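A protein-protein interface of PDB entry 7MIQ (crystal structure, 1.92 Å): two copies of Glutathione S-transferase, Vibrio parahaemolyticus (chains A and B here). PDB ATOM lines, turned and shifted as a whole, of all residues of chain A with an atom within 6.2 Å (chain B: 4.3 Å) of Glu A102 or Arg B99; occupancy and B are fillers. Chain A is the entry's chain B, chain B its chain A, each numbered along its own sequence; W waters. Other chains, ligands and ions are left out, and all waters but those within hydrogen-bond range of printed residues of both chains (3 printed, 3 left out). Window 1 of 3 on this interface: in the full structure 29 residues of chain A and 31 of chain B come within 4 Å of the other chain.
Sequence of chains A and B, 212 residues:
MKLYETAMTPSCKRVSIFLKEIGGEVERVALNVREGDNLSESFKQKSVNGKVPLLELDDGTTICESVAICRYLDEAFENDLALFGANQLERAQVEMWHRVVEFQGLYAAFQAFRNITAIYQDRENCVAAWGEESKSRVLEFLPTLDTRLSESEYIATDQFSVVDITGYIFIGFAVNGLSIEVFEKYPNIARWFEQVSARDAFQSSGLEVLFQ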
ATOM      1  N   ARG A  14     -24.610  18.002  18.705  1.00  0.00           N
ATOM      2  CA  ARG A  14     -23.582  19.038  18.778  1.00  0.00           C
ATOM      3  C   ARG A  14     -23.539  19.665  20.166  1.00  0.00           C
ATOM      4  O   ARG A  14     -22.459  19.864  20.734  1.00  0.00           O
ATOM      5  CB  ARG A  14     -23.828  20.109  17.713  1.00  0.00           C
ATOM      6  CG  ARG A  14     -23.671  19.622  16.276  1.00  0.00           C
ATOM      7  CD  ARG A  14     -24.044  20.712  15.275  1.00  0.00           C
ATOM      8  NE  ARG A  14     -23.015  21.742  15.163  1.00  0.00           N
ATOM      9  CZ  ARG A  14     -23.092  22.788  14.350  1.00  0.00           C
ATOM     10  NH1 ARG A  14     -24.144  22.982  13.569  1.00  0.00           N
ATOM     11  NH2 ARG A  14     -22.086  23.659  14.316  1.00  0.00           N
ATOM     12  N   GLU A  65     -30.336  27.652  17.802  1.00  0.00           N
ATOM     13  CA  GLU A  65     -29.052  27.499  17.105  1.00  0.00           C
ATOM     14  C   GLU A  65     -28.043  26.782  17.994  1.00  0.00           C
ATOM     15  O   GLU A  65     -27.725  27.262  19.088  1.00  0.00           O
ATOM     16  CB  GLU A  65     -28.479  28.845  16.637  1.00  0.00           C
ATOM     17  CG  GLU A  65     -29.248  29.498  15.505  1.00  0.00           C
ATOM     18  CD  GLU A  65     -29.204  28.679  14.226  1.00  0.00           C
ATOM     19  OE1 GLU A  65     -28.161  28.042  13.959  1.00  0.00           O
ATOM     20  OE2 GLU A  65     -30.215  28.668  13.494  1.00  0.00           O
ATOM     21  N   SER A  66     -27.529  25.638  17.527  1.00  0.00           N
ATOM     22  CA  SER A  66     -26.665  24.814  18.370  1.00  0.00           C
ATOM     23  C   SER A  66     -25.438  25.585  18.851  1.00  0.00           C
ATOM     24  O   SER A  66     -25.052  25.473  20.021  1.00  0.00           O
ATOM     25  CB  SER A  66     -26.242  23.550  17.617  1.00  0.00           C
ATOM     26  OG  SER A  66     -25.486  23.862  16.461  1.00  0.00           O
ATOM     27  N   VAL A  67     -24.816  26.374  17.971  1.00  0.00           N
ATOM     28  CA  VAL A  67     -23.597  27.088  18.357  1.00  0.00           C
ATOM     29  C   VAL A  67     -23.906  28.188  19.368  1.00  0.00           C
ATOM     30  O   VAL A  67     -23.109  28.458  20.276  1.00  0.00           O
ATOM     31  CB  VAL A  67     -22.881  27.646  17.113  1.00  0.00           C
ATOM     32  CG1 VAL A  67     -21.664  28.475  17.515  1.00  0.00           C
ATOM     33  CG2 VAL A  67     -22.463  26.508  16.187  1.00  0.00           C
ATOM     34  N   ALA A  68     -25.062  28.843  19.227  1.00  0.00           N
ATOM     35  CA  ALA A  68     -25.461  29.859  20.197  1.00  0.00           C
ATOM     36  C   ALA A  68     -25.697  29.248  21.571  1.00  0.00           C
ATOM     37  O   ALA A  68     -25.340  29.842  22.595  1.00  0.00           O
ATOM     38  CB  ALA A  68     -26.719  30.579  19.709  1.00  0.00           C
ATOM     39  N   GLU A  95     -13.451  31.101  14.864  1.00  0.00           N
ATOM     40  CA  GLU A  95     -14.549  31.664  14.078  1.00  0.00           C
ATOM     41  C   GLU A  95     -14.349  31.411  12.589  1.00  0.00           C
ATOM     42  O   GLU A  95     -15.289  31.019  11.882  1.00  0.00           O
ATOM     43  CB  GLU A  95     -14.673  33.168  14.349  1.00  0.00           C
ATOM     44  CG  GLU A  95     -15.906  33.816  13.721  1.00  0.00           C
ATOM     45  CD  GLU A  95     -17.180  33.471  14.464  1.00  0.00           C
ATOM     46  OE1 GLU A  95     -17.192  33.606  15.704  1.00  0.00           O
ATOM     47  OE2 GLU A  95     -18.156  33.045  13.812  1.00  0.00           O
ATOM     48  N   TRP A  97     -12.407  29.048  10.956  1.00  0.00           N
ATOM     49  CA  TRP A  97     -12.504  27.649  10.558  1.00  0.00           C
ATOM     50  C   TRP A  97     -13.885  27.072  10.839  1.00  0.00           C
ATOM     51  O   TRP A  97     -14.329  26.167  10.123  1.00  0.00           O
ATOM     52  CB  TRP A  97     -11.422  26.828  11.252  1.00  0.00           C
ATOM     53  CG  TRP A  97     -10.099  26.948  10.570  1.00  0.00           C
ATOM     54  CD1 TRP A  97      -9.050  27.739  10.938  1.00  0.00           C
ATOM     55  CD2 TRP A  97      -9.693  26.269   9.379  1.00  0.00           C
ATOM     56  NE1 TRP A  97      -8.008  27.585  10.053  1.00  0.00           N
ATOM     57  CE2 TRP A  97      -8.379  26.685   9.087  1.00  0.00           C
ATOM     58  CE3 TRP A  97     -10.310  25.338   8.538  1.00  0.00           C
ATOM     59  CZ2 TRP A  97      -7.672  26.205   7.987  1.00  0.00           C
ATOM     60  CZ3 TRP A  97      -9.606  24.863   7.442  1.00  0.00           C
ATOM     61  CH2 TRP A  97      -8.299  25.296   7.180  1.00  0.00           C
ATOM     62  N   HIS A  98     -14.587  27.578  11.856  1.00  0.00           N
ATOM     63  CA  HIS A  98     -15.943  27.094  12.101  1.00  0.00           C
ATOM     64  C   HIS A  98     -16.842  27.406  10.913  1.00  0.00           C
ATOM     65  O   HIS A  98     -17.563  26.536  10.416  1.00  0.00           O
ATOM     66  CB  HIS A  98     -16.514  27.704  13.384  1.00  0.00           C
ATOM     67  CG  HIS A  98     -17.462  26.798  14.114  1.00  0.00           C
ATOM     68  ND1 HIS A  98     -18.070  27.155  15.298  1.00  0.00           N
ATOM     69  CD2 HIS A  98     -17.885  25.543  13.838  1.00  0.00           C
ATOM     70  CE1 HIS A  98     -18.835  26.162  15.715  1.00  0.00           C
ATOM     71  NE2 HIS A  98     -18.741  25.170  14.847  1.00  0.00           N
ATOM     72  N   ARG A  99     -16.783  28.642  10.420  1.00  0.00           N
ATOM     73  CA  ARG A  99     -17.628  29.033   9.296  1.00  0.00           C
ATOM     74  C   ARG A  99     -17.232  28.301   8.021  1.00  0.00           C
ATOM     75  O   ARG A  99     -18.094  27.940   7.211  1.00  0.00           O
ATOM     76  CB  ARG A  99     -17.554  30.546   9.107  1.00  0.00           C
ATOM     77  CG  ARG A  99     -18.155  31.290  10.292  1.00  0.00           C
ATOM     78  CD  ARG A  99     -17.962  32.791  10.228  1.00  0.00           C
ATOM     79  NE  ARG A  99     -18.879  33.422  11.172  1.00  0.00           N
ATOM     80  CZ  ARG A  99     -20.118  33.785  10.871  1.00  0.00           C
ATOM     81  NH1 ARG A  99     -20.582  33.696   9.635  1.00  0.00           N
ATOM     82  NH2 ARG A  99     -20.912  34.245  11.833  1.00  0.00           N
ATOM     83  N   VAL A 100     -15.933  28.074   7.827  1.00  0.00           N
ATOM     84  CA  VAL A 100     -15.472  27.316   6.667  1.00  0.00           C
ATOM     85  C   VAL A 100     -16.005  25.891   6.723  1.00  0.00           C
ATOM     86  O   VAL A 100     -16.598  25.392   5.758  1.00  0.00           O
ATOM     87  CB  VAL A 100     -13.934  27.347   6.586  1.00  0.00           C
ATOM     88  CG1 VAL A 100     -13.420  26.293   5.615  1.00  0.00           C
ATOM     89  CG2 VAL A 100     -13.459  28.734   6.176  1.00  0.00           C
ATOM     90  N   VAL A 101     -15.809  25.215   7.858  1.00  0.00           N
ATOM     91  CA  VAL A 101     -16.301  23.846   8.003  1.00  0.00           C
ATOM     92  C   VAL A 101     -17.817  23.803   7.852  1.00  0.00           C
ATOM     93  O   VAL A 101     -18.367  22.898   7.214  1.00  0.00           O
ATOM     94  CB  VAL A 101     -15.848  23.252   9.351  1.00  0.00           C
ATOM     95  CG1 VAL A 101     -16.575  21.942   9.633  1.00  0.00           C
ATOM     96  CG2 VAL A 101     -14.339  23.035   9.359  1.00  0.00           C
ATOM     97  N   GLU A 102     -18.515  24.788   8.423  1.00  0.00           N
ATOM     98  CA  GLU A 102     -19.976  24.772   8.395  1.00  0.00           C
ATOM     99  C   GLU A 102     -20.517  25.013   6.993  1.00  0.00           C
ATOM    100  O   GLU A 102     -21.403  24.287   6.525  1.00  0.00           O
ATOM    101  CB  GLU A 102     -20.529  25.817   9.357  1.00  0.00           C
ATOM    102  CG  GLU A 102     -20.436  25.421  10.808  1.00  0.00           C
ATOM    103  CD  GLU A 102     -21.126  26.423  11.705  1.00  0.00           C
ATOM    104  OE1 GLU A 102     -20.727  27.609  11.701  1.00  0.00           O
ATOM    105  OE2 GLU A 102     -22.075  26.022  12.401  1.00  0.00           O
ATOM    106  N   PHE A 103     -20.015  26.042   6.309  1.00  0.00           N
ATOM    107  CA  PHE A 103     -20.560  26.372   4.995  1.00  0.00           C
ATOM    108  C   PHE A 103     -20.099  25.370   3.946  1.00  0.00           C
ATOM    109  O   PHE A 103     -20.907  24.862   3.157  1.00  0.00           O
ATOM    110  CB  PHE A 103     -20.154  27.789   4.591  1.00  0.00           C
ATOM    111  CG  PHE A 103     -20.813  28.266   3.327  1.00  0.00           C
ATOM    112  CD1 PHE A 103     -22.082  28.823   3.360  1.00  0.00           C
ATOM    113  CD2 PHE A 103     -20.165  28.156   2.106  1.00  0.00           C
ATOM    114  CE1 PHE A 103     -22.694  29.262   2.200  1.00  0.00           C
ATOM    115  CE2 PHE A 103     -20.772  28.594   0.941  1.00  0.00           C
ATOM    116  CZ  PHE A 103     -22.038  29.147   0.989  1.00  0.00           C
ATOM    117  N   GLN A 104     -18.802  25.072   3.926  1.00  0.00           N
ATOM    118  CA  GLN A 104     -18.233  24.223   2.889  1.00  0.00           C
ATOM    119  C   GLN A 104     -18.423  22.742   3.176  1.00  0.00           C
ATOM    120  O   GLN A 104     -18.419  21.935   2.241  1.00  0.00           O
ATOM    121  CB  GLN A 104     -16.746  24.558   2.721  1.00  0.00           C
ATOM    122  CG  GLN A 104     -16.505  26.063   2.553  1.00  0.00           C
ATOM    123  CD  GLN A 104     -15.096  26.414   2.116  1.00  0.00           C
ATOM    124  OE1 GLN A 104     -14.352  25.564   1.630  1.00  0.00           O
ATOM    125  NE2 GLN A 104     -14.722  27.680   2.288  1.00  0.00           N
ATOM    126  N   GLY A 105     -18.613  22.370   4.437  1.00  0.00           N
ATOM    127  CA  GLY A 105     -18.768  20.977   4.789  1.00  0.00           C
ATOM    128  C   GLY A 105     -20.144  20.619   5.316  1.00  0.00           C
ATOM    129  O   GLY A 105     -20.906  19.928   4.636  1.00  0.00           O
ATOM    130  N   LEU A 106     -20.474  21.092   6.521  1.00  0.00           N
ATOM    131  CA  LEU A 106     -21.670  20.614   7.210  1.00  0.00           C
ATOM    132  C   LEU A 106     -22.939  20.940   6.427  1.00  0.00           C
ATOM    133  O   LEU A 106     -23.771  20.059   6.182  1.00  0.00           O
ATOM    134  CB  LEU A 106     -21.738  21.208   8.618  1.00  0.00           C
ATOM    135  CG  LEU A 106     -22.848  20.632   9.503  1.00  0.00           C
ATOM    136  CD1 LEU A 106     -22.703  19.123   9.627  1.00  0.00           C
ATOM    137  CD2 LEU A 106     -22.852  21.282  10.876  1.00  0.00           C
ATOM    138  N   TYR A 107     -23.107  22.205   6.030  1.00  0.00           N
ATOM    139  CA  TYR A 107     -24.342  22.614   5.363  1.00  0.00           C
ATOM    140  C   TYR A 107     -24.502  21.918   4.020  1.00  0.00           C
ATOM    141  O   TYR A 107     -25.609  21.512   3.652  1.00  0.00           O
ATOM    142  CB  TYR A 107     -24.369  24.131   5.170  1.00  0.00           C
ATOM    143  CG  TYR A 107     -24.346  24.932   6.453  1.00  0.00           C
ATOM    144  CD1 TYR A 107     -24.673  24.347   7.669  1.00  0.00           C
ATOM    145  CD2 TYR A 107     -23.996  26.278   6.443  1.00  0.00           C
ATOM    146  CE1 TYR A 107     -24.651  25.077   8.838  1.00  0.00           C
ATOM    147  CE2 TYR A 107     -23.972  27.018   7.608  1.00  0.00           C
ATOM    148  CZ  TYR A 107     -24.301  26.411   8.803  1.00  0.00           C
ATOM    149  OH  TYR A 107     -24.276  27.141   9.967  1.00  0.00           O
ATOM    150  N   ALA A 108     -23.411  21.794   3.263  1.00  0.00           N
ATOM    151  CA  ALA A 108     -23.478  21.070   1.998  1.00  0.00           C
ATOM    152  C   ALA A 108     -23.837  19.606   2.222  1.00  0.00           C
ATOM    153  O   ALA A 108     -24.622  19.030   1.459  1.00  0.00           O
ATOM    154  CB  ALA A 108     -22.150  21.198   1.252  1.00  0.00           C
ATOM    155  N   THR A 166     -17.870  20.159  15.381  1.00  0.00           N
ATOM    156  CA  THR A 166     -18.606  20.369  14.138  1.00  0.00           C
ATOM    157  C   THR A 166     -18.025  19.534  13.002  1.00  0.00           C
ATOM    158  O   THR A 166     -18.768  18.894  12.248  1.00  0.00           O
ATOM    159  CB  THR A 166     -18.597  21.855  13.784  1.00  0.00           C
ATOM    160  OG1 THR A 166     -19.250  22.589  14.828  1.00  0.00           O
ATOM    161  CG2 THR A 166     -19.312  22.109  12.456  1.00  0.00           C
ATOM    162  N   GLU B  95     -25.205  35.543  18.805  1.00  0.00           N
ATOM    163  CA  GLU B  95     -24.862  34.344  18.044  1.00  0.00           C
ATOM    164  C   GLU B  95     -26.098  33.735  17.397  1.00  0.00           C
ATOM    165  O   GLU B  95     -26.076  33.381  16.210  1.00  0.00           O
ATOM    166  CB  GLU B  95     -24.177  33.320  18.953  1.00  0.00           C
ATOM    167  CG  GLU B  95     -23.575  32.129  18.210  1.00  0.00           C
ATOM    168  CD  GLU B  95     -22.300  32.489  17.478  1.00  0.00           C
ATOM    169  OE1 GLU B  95     -21.423  33.129  18.096  1.00  0.00           O
ATOM    170  OE2 GLU B  95     -22.177  32.140  16.286  1.00  0.00           O
ATOM    171  N   MET B  96     -27.189  33.621  18.160  1.00  0.00           N
ATOM    172  CA  MET B  96     -28.422  33.046  17.627  1.00  0.00           C
ATOM    173  C   MET B  96     -28.952  33.858  16.451  1.00  0.00           C
ATOM    174  O   MET B  96     -29.186  33.319  15.362  1.00  0.00           O
ATOM    175  CB  MET B  96     -29.476  32.955  18.731  1.00  0.00           C
ATOM    176  CG  MET B  96     -30.878  32.685  18.214  1.00  0.00           C
ATOM    177  SD  MET B  96     -32.109  32.567  19.531  1.00  0.00           S
ATOM    178  CE  MET B  96     -31.997  34.189  20.283  1.00  0.00           C
ATOM    179  N   TRP B  97     -29.160  35.162  16.654  1.00  0.00           N
ATOM    180  CA  TRP B  97     -29.768  35.970  15.599  1.00  0.00           C
ATOM    181  C   TRP B  97     -28.814  36.202  14.433  1.00  0.00           C
ATOM    182  O   TRP B  97     -29.266  36.359  13.292  1.00  0.00           O
ATOM    183  CB  TRP B  97     -30.259  37.299  16.167  1.00  0.00           C
ATOM    184  CG  TRP B  97     -31.607  37.167  16.810  1.00  0.00           C
ATOM    185  CD1 TRP B  97     -31.880  37.092  18.144  1.00  0.00           C
ATOM    186  CD2 TRP B  97     -32.865  37.059  16.134  1.00  0.00           C
ATOM    187  NE1 TRP B  97     -33.236  36.954  18.342  1.00  0.00           N
ATOM    188  CE2 TRP B  97     -33.861  36.934  17.123  1.00  0.00           C
ATOM    189  CE3 TRP B  97     -33.245  37.062  14.788  1.00  0.00           C
ATOM    190  CZ2 TRP B  97     -35.215  36.815  16.807  1.00  0.00           C
ATOM    191  CZ3 TRP B  97     -34.591  36.944  14.475  1.00  0.00           C
ATOM    192  CH2 TRP B  97     -35.558  36.822  15.481  1.00  0.00           C
ATOM    193  N   HIS B  98     -27.501  36.235  14.685  1.00  0.00           N
ATOM    194  CA  HIS B  98     -26.563  36.351  13.573  1.00  0.00           C
ATOM    195  C   HIS B  98     -26.706  35.169  12.629  1.00  0.00           C
ATOM    196  O   HIS B  98     -26.777  35.345  11.410  1.00  0.00           O
ATOM    197  CB  HIS B  98     -25.119  36.458  14.075  1.00  0.00           C
ATOM    198  CG  HIS B  98     -24.248  37.315  13.208  1.00  0.00           C
ATOM    199  ND1 HIS B  98     -22.923  37.566  13.495  1.00  0.00           N
ATOM    200  CD2 HIS B  98     -24.519  37.989  12.065  1.00  0.00           C
ATOM    201  CE1 HIS B  98     -22.413  38.352  12.563  1.00  0.00           C
ATOM    202  NE2 HIS B  98     -23.362  38.627  11.684  1.00  0.00           N
ATOM    203  N   ARG B  99     -26.790  33.958  13.180  1.00  0.00           N
ATOM    204  CA  ARG B  99     -26.893  32.765  12.346  1.00  0.00           C
ATOM    205  C   ARG B  99     -28.241  32.689  11.640  1.00  0.00           C
ATOM    206  O   ARG B  99     -28.316  32.260  10.481  1.00  0.00           O
ATOM    207  CB  ARG B  99     -26.645  31.523  13.202  1.00  0.00           C
ATOM    208  CG  ARG B  99     -25.192  31.418  13.629  1.00  0.00           C
ATOM    209  CD  ARG B  99     -24.912  30.297  14.612  1.00  0.00           C
ATOM    210  NE  ARG B  99     -23.469  30.104  14.707  1.00  0.00           N
ATOM    211  CZ  ARG B  99     -22.775  29.291  13.921  1.00  0.00           C
ATOM    212  NH1 ARG B  99     -23.372  28.500  13.046  1.00  0.00           N
ATOM    213  NH2 ARG B  99     -21.447  29.279  14.008  1.00  0.00           N
ATOM    214  N   VAL B 100     -29.314  33.103  12.315  1.00  0.00           N
ATOM    215  CA  VAL B 100     -30.632  33.125  11.679  1.00  0.00           C
ATOM    216  C   VAL B 100     -30.633  34.089  10.498  1.00  0.00           C
ATOM    217  O   VAL B 100     -31.059  33.741   9.389  1.00  0.00           O
ATOM    218  CB  VAL B 100     -31.717  33.486  12.709  1.00  0.00           C
ATOM    219  CG1 VAL B 100     -33.027  33.793  12.012  1.00  0.00           C
ATOM    220  CG2 VAL B 100     -31.901  32.349  13.706  1.00  0.00           C
ATOM    221  N   VAL B 101     -30.138  35.314  10.711  1.00  0.00           N
ATOM    222  CA  VAL B 101     -30.106  36.297   9.626  1.00  0.00           C
ATOM    223  C   VAL B 101     -29.191  35.827   8.494  1.00  0.00           C
ATOM    224  O   VAL B 101     -29.506  36.002   7.310  1.00  0.00           O
ATOM    225  CB  VAL B 101     -29.683  37.680  10.164  1.00  0.00           C
ATOM    226  CG1 VAL B 101     -29.388  38.638   9.018  1.00  0.00           C
ATOM    227  CG2 VAL B 101     -30.767  38.263  11.073  1.00  0.00           C
ATOM    228  N   GLU B 102     -28.047  35.230   8.833  1.00  0.00           N
ATOM    229  CA  GLU B 102     -27.076  34.795   7.796  1.00  0.00           C
ATOM    230  C   GLU B 102     -27.651  33.630   6.977  1.00  0.00           C
ATOM    231  O   GLU B 102     -27.758  33.790   5.772  1.00  0.00           O
ATOM    232  CB  GLU B 102     -25.724  34.440   8.402  1.00  0.00           C
ATOM    233  CG  GLU B 102     -24.877  35.645   8.723  1.00  0.00           C
ATOM    234  CD  GLU B 102     -23.582  35.274   9.417  1.00  0.00           C
ATOM    235  OE1 GLU B 102     -23.635  34.526  10.412  1.00  0.00           O
ATOM    236  OE2 GLU B 102     -22.538  35.726   8.957  1.00  0.00           O
ATOM    237  N   PHE B 103     -28.052  32.520   7.604  1.00  0.00           N
ATOM    238  CA  PHE B 103     -28.601  31.393   6.842  1.00  0.00           C
ATOM    239  C   PHE B 103     -29.910  31.758   6.150  1.00  0.00           C
ATOM    240  O   PHE B 103     -30.029  31.658   4.924  1.00  0.00           O
ATOM    241  CB  PHE B 103     -28.837  30.176   7.736  1.00  0.00           C
ATOM    242  CG  PHE B 103     -29.090  28.908   6.970  1.00  0.00           C
ATOM    243  CD1 PHE B 103     -28.046  28.244   6.345  1.00  0.00           C
ATOM    244  CD2 PHE B 103     -30.368  28.383   6.868  1.00  0.00           C
ATOM    245  CE1 PHE B 103     -28.270  27.079   5.637  1.00  0.00           C
ATOM    246  CE2 PHE B 103     -30.600  27.217   6.160  1.00  0.00           C
ATOM    247  CZ  PHE B 103     -29.550  26.565   5.543  1.00  0.00           C
HETATM  248  O   HOH W   1     -20.820  35.180   6.955  1.00  0.00           O
HETATM  249  O   HOH W   2     -20.811  33.998  14.802  1.00  0.00           O
HETATM  250  O   HOH W   3     -19.779  31.268  15.194  1.00  0.00           O
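The guanidinium group (NH1) of Arg B99 sits at hydrogen-bond distance from the side-chain hydroxyl (OH) of Tyr A107 (3.5 Å). OE2 of Glu A102 lies within salt-bridge range of NH1 of Arg B99 (2.9 Å). The side-chain carboxylate of Glu B102 lies within salt-bridge range of the guanidinium group of Arg A99, 2.9 Å away.
Among the printed residues, pairs that only touch across the chains: Ala A68 with Met B96 (3.4 Å), Val A67 with Arg B99 (3.5 Å), Ala A68 with Glu B95 (3.6 Å), Glu A65 with Met B96 (3.8 Å), Glu A65 with Arg B99 (3.9 Å) and Val A67 with Glu B95 (3.9 Å).
Arg A99 touches Glu B102, and with the chains exchanged Glu A102 touches Arg B99. 8 positions are printed for both chains. Of the 9 pairs that touch across the chains among the printed residues, 2 have their exchanged pair printed and touching as well.
OE2 of Glu A102 lies within salt-bridge range of NH2 of Arg A14 (3.0 Å). OE2 of Glu B95 lies within salt-bridge range of NE of Arg B99 (2.9 Å). The guanidinium group of Arg A99 is in salt-bridge range of the side-chain carboxylate of Glu A95, 2.8 Å away. The backbone carbonyl oxygen (O) of Glu A102 sits at hydrogen-bond distance from the backbone NH (N) of Tyr A107.
Water W1 bridges the side-chain carboxylate (OE2) of Glu B102 and the guanidinium group (NH1) of Arg A99. Water W2 lies within hydrogen-bond range of the side-chain carboxylate (OE2) of Glu B95 (2.7 Å), the guanidinium group (NH2) of Arg A99 (3.0 Å) and the side-chain carboxylate (OE2) of Glu A95 (3.0 Å). Water W3 lies within hydrogen-bond range of the side-chain carboxylate (OE2) of Glu A95 (2.8 Å), the side-chain carboxylate (OE2) of Glu B95 (2.8 Å) and the guanidinium group (NH2) of Arg B99 (2.9 Å).
Hydrophobic or aromatic side chains of chain A within 4 Å of the printed part of chain B: Val A67, Ala A68 and Tyr A107. Of the 9 printed residues of chain B, 4 touch a printed residue of chain A. Hydrophobic or aromatic side chains of chain B that line the printed part of chain A: Met B96. Among the printed residues, 9 pairs touch across the chains. Among the printed residues, Asp or Glu carboxylates within 4 Å of a Lys or Arg side-chain nitrogen of the other chain: Arg A99 with Glu B102 and Glu A102 with Arg B99.
Of the printed residues of chain B, Glu A65 touches Met B96 (3.8 Å) and Arg B99 (3.9 Å). Printed residues of chain B within 4 Å of Val A67: Glu B95 (3.9 Å) and Arg B99 (3.5 Å). Of the printed residues of chain B, Ala A68 touches Glu B95 (3.6 Å) and Met B96 (3.4 Å). Val A100 touches none of the printed residues of chain B. Glu A102 touches just one residue of chain B: Arg B99. Arg B99 touches four residues of chain A. Val B100 touches none of the printed residues of chain A. The nearest residue of chain A that does not touch Arg B99 is His A98 (4.2 Å). The nearest printed residue of chain B that does not touch Val A67 is Met B96 (6.5 Å).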
